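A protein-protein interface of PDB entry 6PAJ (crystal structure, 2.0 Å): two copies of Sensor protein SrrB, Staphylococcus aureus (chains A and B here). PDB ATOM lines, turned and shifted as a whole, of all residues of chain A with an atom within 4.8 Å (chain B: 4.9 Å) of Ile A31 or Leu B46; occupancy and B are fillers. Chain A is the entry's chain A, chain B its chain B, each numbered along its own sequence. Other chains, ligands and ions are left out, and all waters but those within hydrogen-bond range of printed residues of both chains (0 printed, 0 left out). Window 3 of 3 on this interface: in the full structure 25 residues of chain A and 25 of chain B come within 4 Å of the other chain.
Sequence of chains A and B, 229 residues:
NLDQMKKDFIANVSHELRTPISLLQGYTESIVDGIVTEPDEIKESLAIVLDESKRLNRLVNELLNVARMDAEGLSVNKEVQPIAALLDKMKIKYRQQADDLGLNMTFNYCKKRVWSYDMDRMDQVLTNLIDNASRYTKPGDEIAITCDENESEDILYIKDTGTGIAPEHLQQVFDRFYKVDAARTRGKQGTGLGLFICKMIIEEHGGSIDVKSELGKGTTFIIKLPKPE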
ATOM      1  N   TYR A  27       5.837  -0.904 -14.389  1.00  0.00           N
ATOM      2  CA  TYR A  27       6.775  -1.204 -15.448  1.00  0.00           C
ATOM      3  C   TYR A  27       7.591  -2.464 -15.091  1.00  0.00           C
ATOM      4  O   TYR A  27       7.940  -3.256 -15.982  1.00  0.00           O
ATOM      5  CB  TYR A  27       7.655   0.013 -15.750  1.00  0.00           C
ATOM      6  CG  TYR A  27       7.119   0.937 -16.823  1.00  0.00           C
ATOM      7  CD1 TYR A  27       7.416   0.737 -18.170  1.00  0.00           C
ATOM      8  CD2 TYR A  27       6.322   2.024 -16.507  1.00  0.00           C
ATOM      9  CE1 TYR A  27       6.893   1.559 -19.165  1.00  0.00           C
ATOM     10  CE2 TYR A  27       5.793   2.847 -17.489  1.00  0.00           C
ATOM     11  CZ  TYR A  27       6.087   2.636 -18.829  1.00  0.00           C
ATOM     12  OH  TYR A  27       5.573   3.493 -19.791  1.00  0.00           O
ATOM     13  N   THR A  28       7.883  -2.671 -13.802  1.00  0.00           N
ATOM     14  CA  THR A  28       8.581  -3.876 -13.314  1.00  0.00           C
ATOM     15  C   THR A  28       7.676  -5.110 -13.464  1.00  0.00           C
ATOM     16  O   THR A  28       8.087  -6.163 -14.029  1.00  0.00           O
ATOM     17  CB  THR A  28       9.062  -3.669 -11.868  1.00  0.00           C
ATOM     18  OG1 THR A  28       9.914  -2.522 -11.819  1.00  0.00           O
ATOM     19  CG2 THR A  28       9.872  -4.819 -11.327  1.00  0.00           C
ATOM     20  N   GLU A  29       6.454  -4.986 -12.999  1.00  0.00           N
ATOM     21  CA  GLU A  29       5.512  -6.100 -12.986  1.00  0.00           C
ATOM     22  C   GLU A  29       5.287  -6.650 -14.408  1.00  0.00           C
ATOM     23  O   GLU A  29       5.085  -7.887 -14.558  1.00  0.00           O
ATOM     24  CB  GLU A  29       4.196  -5.664 -12.345  1.00  0.00           C
ATOM     25  CG  GLU A  29       3.183  -6.780 -12.160  1.00  0.00           C
ATOM     26  CD  GLU A  29       2.266  -6.574 -10.965  1.00  0.00           C
ATOM     27  OE1 GLU A  29       1.784  -5.444 -10.806  1.00  0.00           O
ATOM     28  OE2 GLU A  29       2.088  -7.520 -10.152  1.00  0.00           O
ATOM     29  N   SER A  30       5.271  -5.778 -15.430  1.00  0.00           N
ATOM     30  CA  SER A  30       5.046  -6.210 -16.844  1.00  0.00           C
ATOM     31  C   SER A  30       6.169  -7.143 -17.297  1.00  0.00           C
ATOM     32  O   SER A  30       5.929  -8.099 -18.059  1.00  0.00           O
ATOM     33  CB  SER A  30       4.942  -5.045 -17.800  1.00  0.00           C
ATOM     34  OG  SER A  30       3.742  -4.327 -17.621  1.00  0.00           O
ATOM     35  N   ILE A  31       7.371  -6.868 -16.806  1.00  0.00           N
ATOM     36  CA  ILE A  31       8.542  -7.707 -17.070  1.00  0.00           C
ATOM     37  C   ILE A  31       8.437  -9.009 -16.267  1.00  0.00           C
ATOM     38  O   ILE A  31       8.682 -10.110 -16.819  1.00  0.00           O
ATOM     39  CB  ILE A  31       9.860  -6.989 -16.740  1.00  0.00           C
ATOM     40  CG1 ILE A  31       9.932  -5.584 -17.333  1.00  0.00           C
ATOM     41  CG2 ILE A  31      11.044  -7.843 -17.185  1.00  0.00           C
ATOM     42  CD1 ILE A  31       9.978  -5.578 -18.826  1.00  0.00           C
ATOM     43  N   VAL A  32       8.120  -8.930 -14.970  1.00  0.00           N
ATOM     44  CA  VAL A  32       8.112 -10.168 -14.208  1.00  0.00           C
ATOM     45  C   VAL A  32       6.981 -11.067 -14.749  1.00  0.00           C
ATOM     46  O   VAL A  32       7.191 -12.267 -14.833  1.00  0.00           O
ATOM     47  CB  VAL A  32       8.118 -10.069 -12.661  1.00  0.00           C
ATOM     48  CG1 VAL A  32       8.784  -8.810 -12.118  1.00  0.00           C
ATOM     49  CG2 VAL A  32       6.805 -10.359 -11.959  1.00  0.00           C
ATOM     50  N   ASP A  33       5.853 -10.507 -15.182  1.00  0.00           N
ATOM     51  CA  ASP A  33       4.682 -11.310 -15.588  1.00  0.00           C
ATOM     52  C   ASP A  33       4.851 -11.838 -17.024  1.00  0.00           C
ATOM     53  O   ASP A  33       3.966 -12.495 -17.516  1.00  0.00           O
ATOM     54  CB  ASP A  33       3.386 -10.504 -15.444  1.00  0.00           C
ATOM     55  CG  ASP A  33       2.919 -10.341 -14.001  1.00  0.00           C
ATOM     56  OD1 ASP A  33       3.559 -10.930 -13.099  1.00  0.00           O
ATOM     57  OD2 ASP A  33       1.920  -9.617 -13.773  1.00  0.00           O
ATOM     58  N   GLY A  34       5.946 -11.517 -17.698  1.00  0.00           N
ATOM     59  CA  GLY A  34       6.236 -11.973 -19.072  1.00  0.00           C
ATOM     60  C   GLY A  34       5.447 -11.243 -20.161  1.00  0.00           C
ATOM     61  O   GLY A  34       5.325 -11.763 -21.287  1.00  0.00           O
ATOM     62  N   VAL A  36       6.263  -7.917 -21.114  1.00  0.00           N
ATOM     63  CA  VAL A  36       7.296  -7.192 -21.826  1.00  0.00           C
ATOM     64  C   VAL A  36       8.561  -8.056 -21.804  1.00  0.00           C
ATOM     65  O   VAL A  36       9.104  -8.346 -20.733  1.00  0.00           O
ATOM     66  CB  VAL A  36       7.522  -5.791 -21.219  1.00  0.00           C
ATOM     67  CG1 VAL A  36       8.815  -5.148 -21.685  1.00  0.00           C
ATOM     68  CG2 VAL A  36       6.355  -4.856 -21.521  1.00  0.00           C
ATOM     69  N   ILE A  42      12.608  -4.332 -22.650  1.00  0.00           N
ATOM     70  CA  ILE A  42      12.994  -4.447 -21.243  1.00  0.00           C
ATOM     71  C   ILE A  42      13.992  -3.339 -20.894  1.00  0.00           C
ATOM     72  O   ILE A  42      13.933  -2.796 -19.798  1.00  0.00           O
ATOM     73  CB  ILE A  42      13.557  -5.849 -20.954  1.00  0.00           C
ATOM     74  CG1 ILE A  42      12.451  -6.900 -21.030  1.00  0.00           C
ATOM     75  CG2 ILE A  42      14.281  -5.885 -19.616  1.00  0.00           C
ATOM     76  CD1 ILE A  42      12.944  -8.287 -21.372  1.00  0.00           C
ATOM     77  N   SER A  45      12.115  -0.149 -20.386  1.00  0.00           N
ATOM     78  CA  SER A  45      11.310  -0.232 -19.189  1.00  0.00           C
ATOM     79  C   SER A  45      12.200  -0.051 -17.949  1.00  0.00           C
ATOM     80  O   SER A  45      11.799   0.619 -16.995  1.00  0.00           O
ATOM     81  CB  SER A  45      10.544  -1.550 -19.133  1.00  0.00           C
ATOM     82  OG  SER A  45       9.432  -1.566 -20.016  1.00  0.00           O
ATOM     83  N   LEU A  46      13.391  -0.662 -17.929  1.00  0.00           N
ATOM     84  CA  LEU A  46      14.245  -0.594 -16.738  1.00  0.00           C
ATOM     85  C   LEU A  46      14.903   0.789 -16.632  1.00  0.00           C
ATOM     86  O   LEU A  46      15.160   1.262 -15.501  1.00  0.00           O
ATOM     87  CB  LEU A  46      15.277  -1.722 -16.794  1.00  0.00           C
ATOM     88  CG  LEU A  46      14.731  -3.151 -16.642  1.00  0.00           C
ATOM     89  CD1 LEU A  46      15.852  -4.155 -16.753  1.00  0.00           C
ATOM     90  CD2 LEU A  46      13.981  -3.339 -15.342  1.00  0.00           C
ATOM     91  N   ILE B  31      21.107  -5.044 -13.580  1.00  0.00           N
ATOM     92  CA  ILE B  31      20.566  -5.594 -14.849  1.00  0.00           C
ATOM     93  C   ILE B  31      20.881  -4.636 -16.004  1.00  0.00           C
ATOM     94  O   ILE B  31      21.381  -5.080 -17.027  1.00  0.00           O
ATOM     95  CB  ILE B  31      19.054  -5.856 -14.762  1.00  0.00           C
ATOM     96  CG1 ILE B  31      18.732  -6.899 -13.686  1.00  0.00           C
ATOM     97  CG2 ILE B  31      18.495  -6.236 -16.138  1.00  0.00           C
ATOM     98  CD1 ILE B  31      17.295  -6.932 -13.259  1.00  0.00           C
ATOM     99  N   ILE B  42      18.447 -12.643 -13.497  1.00  0.00           N
ATOM    100  CA  ILE B  42      17.676 -11.480 -13.906  1.00  0.00           C
ATOM    101  C   ILE B  42      16.276 -11.620 -13.301  1.00  0.00           C
ATOM    102  O   ILE B  42      15.797 -10.704 -12.639  1.00  0.00           O
ATOM    103  CB  ILE B  42      17.675 -11.282 -15.437  1.00  0.00           C
ATOM    104  CG1 ILE B  42      19.071 -10.883 -15.940  1.00  0.00           C
ATOM    105  CG2 ILE B  42      16.635 -10.249 -15.845  1.00  0.00           C
ATOM    106  CD1 ILE B  42      19.206 -10.867 -17.454  1.00  0.00           C
ATOM    107  N   LYS B  43      15.660 -12.780 -13.426  1.00  0.00           N
ATOM    108  CA  LYS B  43      14.294 -12.941 -12.876  1.00  0.00           C
ATOM    109  C   LYS B  43      14.250 -12.800 -11.339  1.00  0.00           C
ATOM    110  O   LYS B  43      13.308 -12.230 -10.761  1.00  0.00           O
ATOM    111  CB  LYS B  43      13.732 -14.298 -13.285  1.00  0.00           C
ATOM    112  CG  LYS B  43      13.356 -14.399 -14.753  1.00  0.00           C
ATOM    113  CD  LYS B  43      12.905 -15.791 -15.146  1.00  0.00           C
ATOM    114  CE  LYS B  43      13.589 -16.305 -16.395  1.00  0.00           C
ATOM    115  NZ  LYS B  43      12.749 -16.085 -17.590  1.00  0.00           N
ATOM    116  N   GLU B  44      15.218 -13.354 -10.636  1.00  0.00           N
ATOM    117  CA  GLU B  44      15.206 -13.271  -9.187  1.00  0.00           C
ATOM    118  C   GLU B  44      15.411 -11.806  -8.780  1.00  0.00           C
ATOM    119  O   GLU B  44      14.808 -11.343  -7.790  1.00  0.00           O
ATOM    120  CB  GLU B  44      16.284 -14.169  -8.566  1.00  0.00           C
ATOM    121  CG  GLU B  44      15.959 -15.655  -8.649  1.00  0.00           C
ATOM    122  CD  GLU B  44      17.082 -16.608  -8.240  1.00  0.00           C
ATOM    123  OE1 GLU B  44      17.970 -16.176  -7.467  1.00  0.00           O
ATOM    124  OE2 GLU B  44      17.067 -17.783  -8.688  1.00  0.00           O
ATOM    125  N   SER B  45      16.247 -11.099  -9.556  1.00  0.00           N
ATOM    126  CA  SER B  45      16.535  -9.709  -9.299  1.00  0.00           C
ATOM    127  C   SER B  45      15.263  -8.867  -9.455  1.00  0.00           C
ATOM    128  O   SER B  45      14.977  -8.037  -8.608  1.00  0.00           O
ATOM    129  CB  SER B  45      17.647  -9.205 -10.196  1.00  0.00           C
ATOM    130  OG  SER B  45      18.832  -9.955  -9.967  1.00  0.00           O
ATOM    131  N   LEU B  46      14.513  -9.105 -10.535  1.00  0.00           N
ATOM    132  CA  LEU B  46      13.304  -8.328 -10.842  1.00  0.00           C
ATOM    133  C   LEU B  46      12.196  -8.621  -9.833  1.00  0.00           C
ATOM    134  O   LEU B  46      11.465  -7.692  -9.481  1.00  0.00           O
ATOM    135  CB  LEU B  46      12.853  -8.611 -12.279  1.00  0.00           C
ATOM    136  CG  LEU B  46      13.704  -7.890 -13.323  1.00  0.00           C
ATOM    137  CD1 LEU B  46      13.243  -8.207 -14.726  1.00  0.00           C
ATOM    138  CD2 LEU B  46      13.705  -6.387 -13.079  1.00  0.00           C
ATOM    139  N   ALA B  47      12.099  -9.861  -9.348  1.00  0.00           N
ATOM    140  CA  ALA B  47      11.118 -10.182  -8.315  1.00  0.00           C
ATOM    141  C   ALA B  47      11.378  -9.340  -7.059  1.00  0.00           C
ATOM    142  O   ALA B  47      10.442  -8.879  -6.412  1.00  0.00           O
ATOM    143  CB  ALA B  47      11.138 -11.656  -7.988  1.00  0.00           C
ATOM    144  N   ILE B  48      12.648  -9.179  -6.701  1.00  0.00           N
ATOM    145  CA  ILE B  48      13.000  -8.329  -5.606  1.00  0.00           C
ATOM    146  C   ILE B  48      12.669  -6.869  -5.939  1.00  0.00           C
ATOM    147  O   ILE B  48      12.172  -6.132  -5.041  1.00  0.00           O
ATOM    148  CB  ILE B  48      14.470  -8.519  -5.191  1.00  0.00           C
ATOM    149  CG1 ILE B  48      14.701  -9.928  -4.627  1.00  0.00           C
ATOM    150  CG2 ILE B  48      14.884  -7.450  -4.201  1.00  0.00           C
ATOM    151  CD1 ILE B  48      16.186 -10.303  -4.510  1.00  0.00           C
ATOM    152  N   VAL B  49      13.012  -6.405  -7.146  1.00  0.00           N
ATOM    153  CA  VAL B  49      12.660  -5.042  -7.495  1.00  0.00           C
ATOM    154  C   VAL B  49      11.150  -4.801  -7.259  1.00  0.00           C
ATOM    155  O   VAL B  49      10.733  -3.815  -6.630  1.00  0.00           O
ATOM    156  CB  VAL B  49      13.061  -4.673  -8.925  1.00  0.00           C
ATOM    157  CG1 VAL B  49      12.470  -3.319  -9.295  1.00  0.00           C
ATOM    158  CG2 VAL B  49      14.570  -4.654  -9.098  1.00  0.00           C
ATOM    159  N   LEU B  50      10.323  -5.732  -7.705  1.00  0.00           N
ATOM    160  CA  LEU B  50       8.847  -5.577  -7.638  1.00  0.00           C
ATOM    161  C   LEU B  50       8.415  -5.593  -6.177  1.00  0.00           C
ATOM    162  O   LEU B  50       7.615  -4.759  -5.782  1.00  0.00           O
ATOM    163  CB  LEU B  50       8.218  -6.754  -8.396  1.00  0.00           C
ATOM    164  CG  LEU B  50       6.886  -6.571  -9.120  1.00  0.00           C
ATOM    165  CD1 LEU B  50       6.093  -7.877  -9.098  1.00  0.00           C
ATOM    166  CD2 LEU B  50       6.061  -5.406  -8.630  1.00  0.00           C
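Among the printed residues, merely in contact across the chains: Ile A31 with Leu B46 (3.3 Å), Leu A46 with Ile B31 (3.4 Å), Thr A28 with Val B49 (3.6 Å), Thr A28 with Leu B50 (3.8 Å), Thr A28 with Leu B46 (3.8 Å), Leu A46 with Leu B46 (3.8 Å), Val A32 with Leu B50 (3.9 Å) and Val A32 with Leu B46 (3.9 Å).
Of the printed residues of chain B, Ile A31 touches Leu B46. Gly A34 touches none of the printed residues of chain B. Of the printed residues of chain B, Leu A46 touches Ile B31 and Leu B46. Of the printed residues of chain A, Ile B31 touches Leu A46 (3.4 Å). Lys B43 touches none of the printed residues of chain A. Of the printed residues of chain A, Leu B46 touches Thr A28 (3.8 Å), Ile A31 (3.3 Å), Val A32 (3.9 Å) and Leu A46 (3.8 Å). The nearest printed residue of chain B that does not touch Ile A31 is Ile B42 (6.2 Å). The nearest printed residue of chain A that does not touch Leu B46 is Ile A42 (5.5 Å).
Hydrophobic or aromatic side chains of chain A that line the printed part of chain B: Ile A31, Val A32 and Leu A46. Of the 10 printed residues of chain B, 4 touch a printed residue of chain A. Hydrophobic or aromatic side chains of chain B within 4 Å of the printed part of chain A: Ile B31, Leu B46, Val B49 and Leu B50. Among the printed residues, no Asp or Glu carboxylate lies within 4 Å of a Lys or Arg side-chain nitrogen of the other chain.
Ile A31 touches Leu B46, and with the chains exchanged Leu A46 touches Ile B31. Leu B46 touches its own counterpart, Leu A46. 4 positions are printed for both chains. Of the 8 pairs that touch across the chains among the printed residues, 3 have their exchanged pair printed and touching as well.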
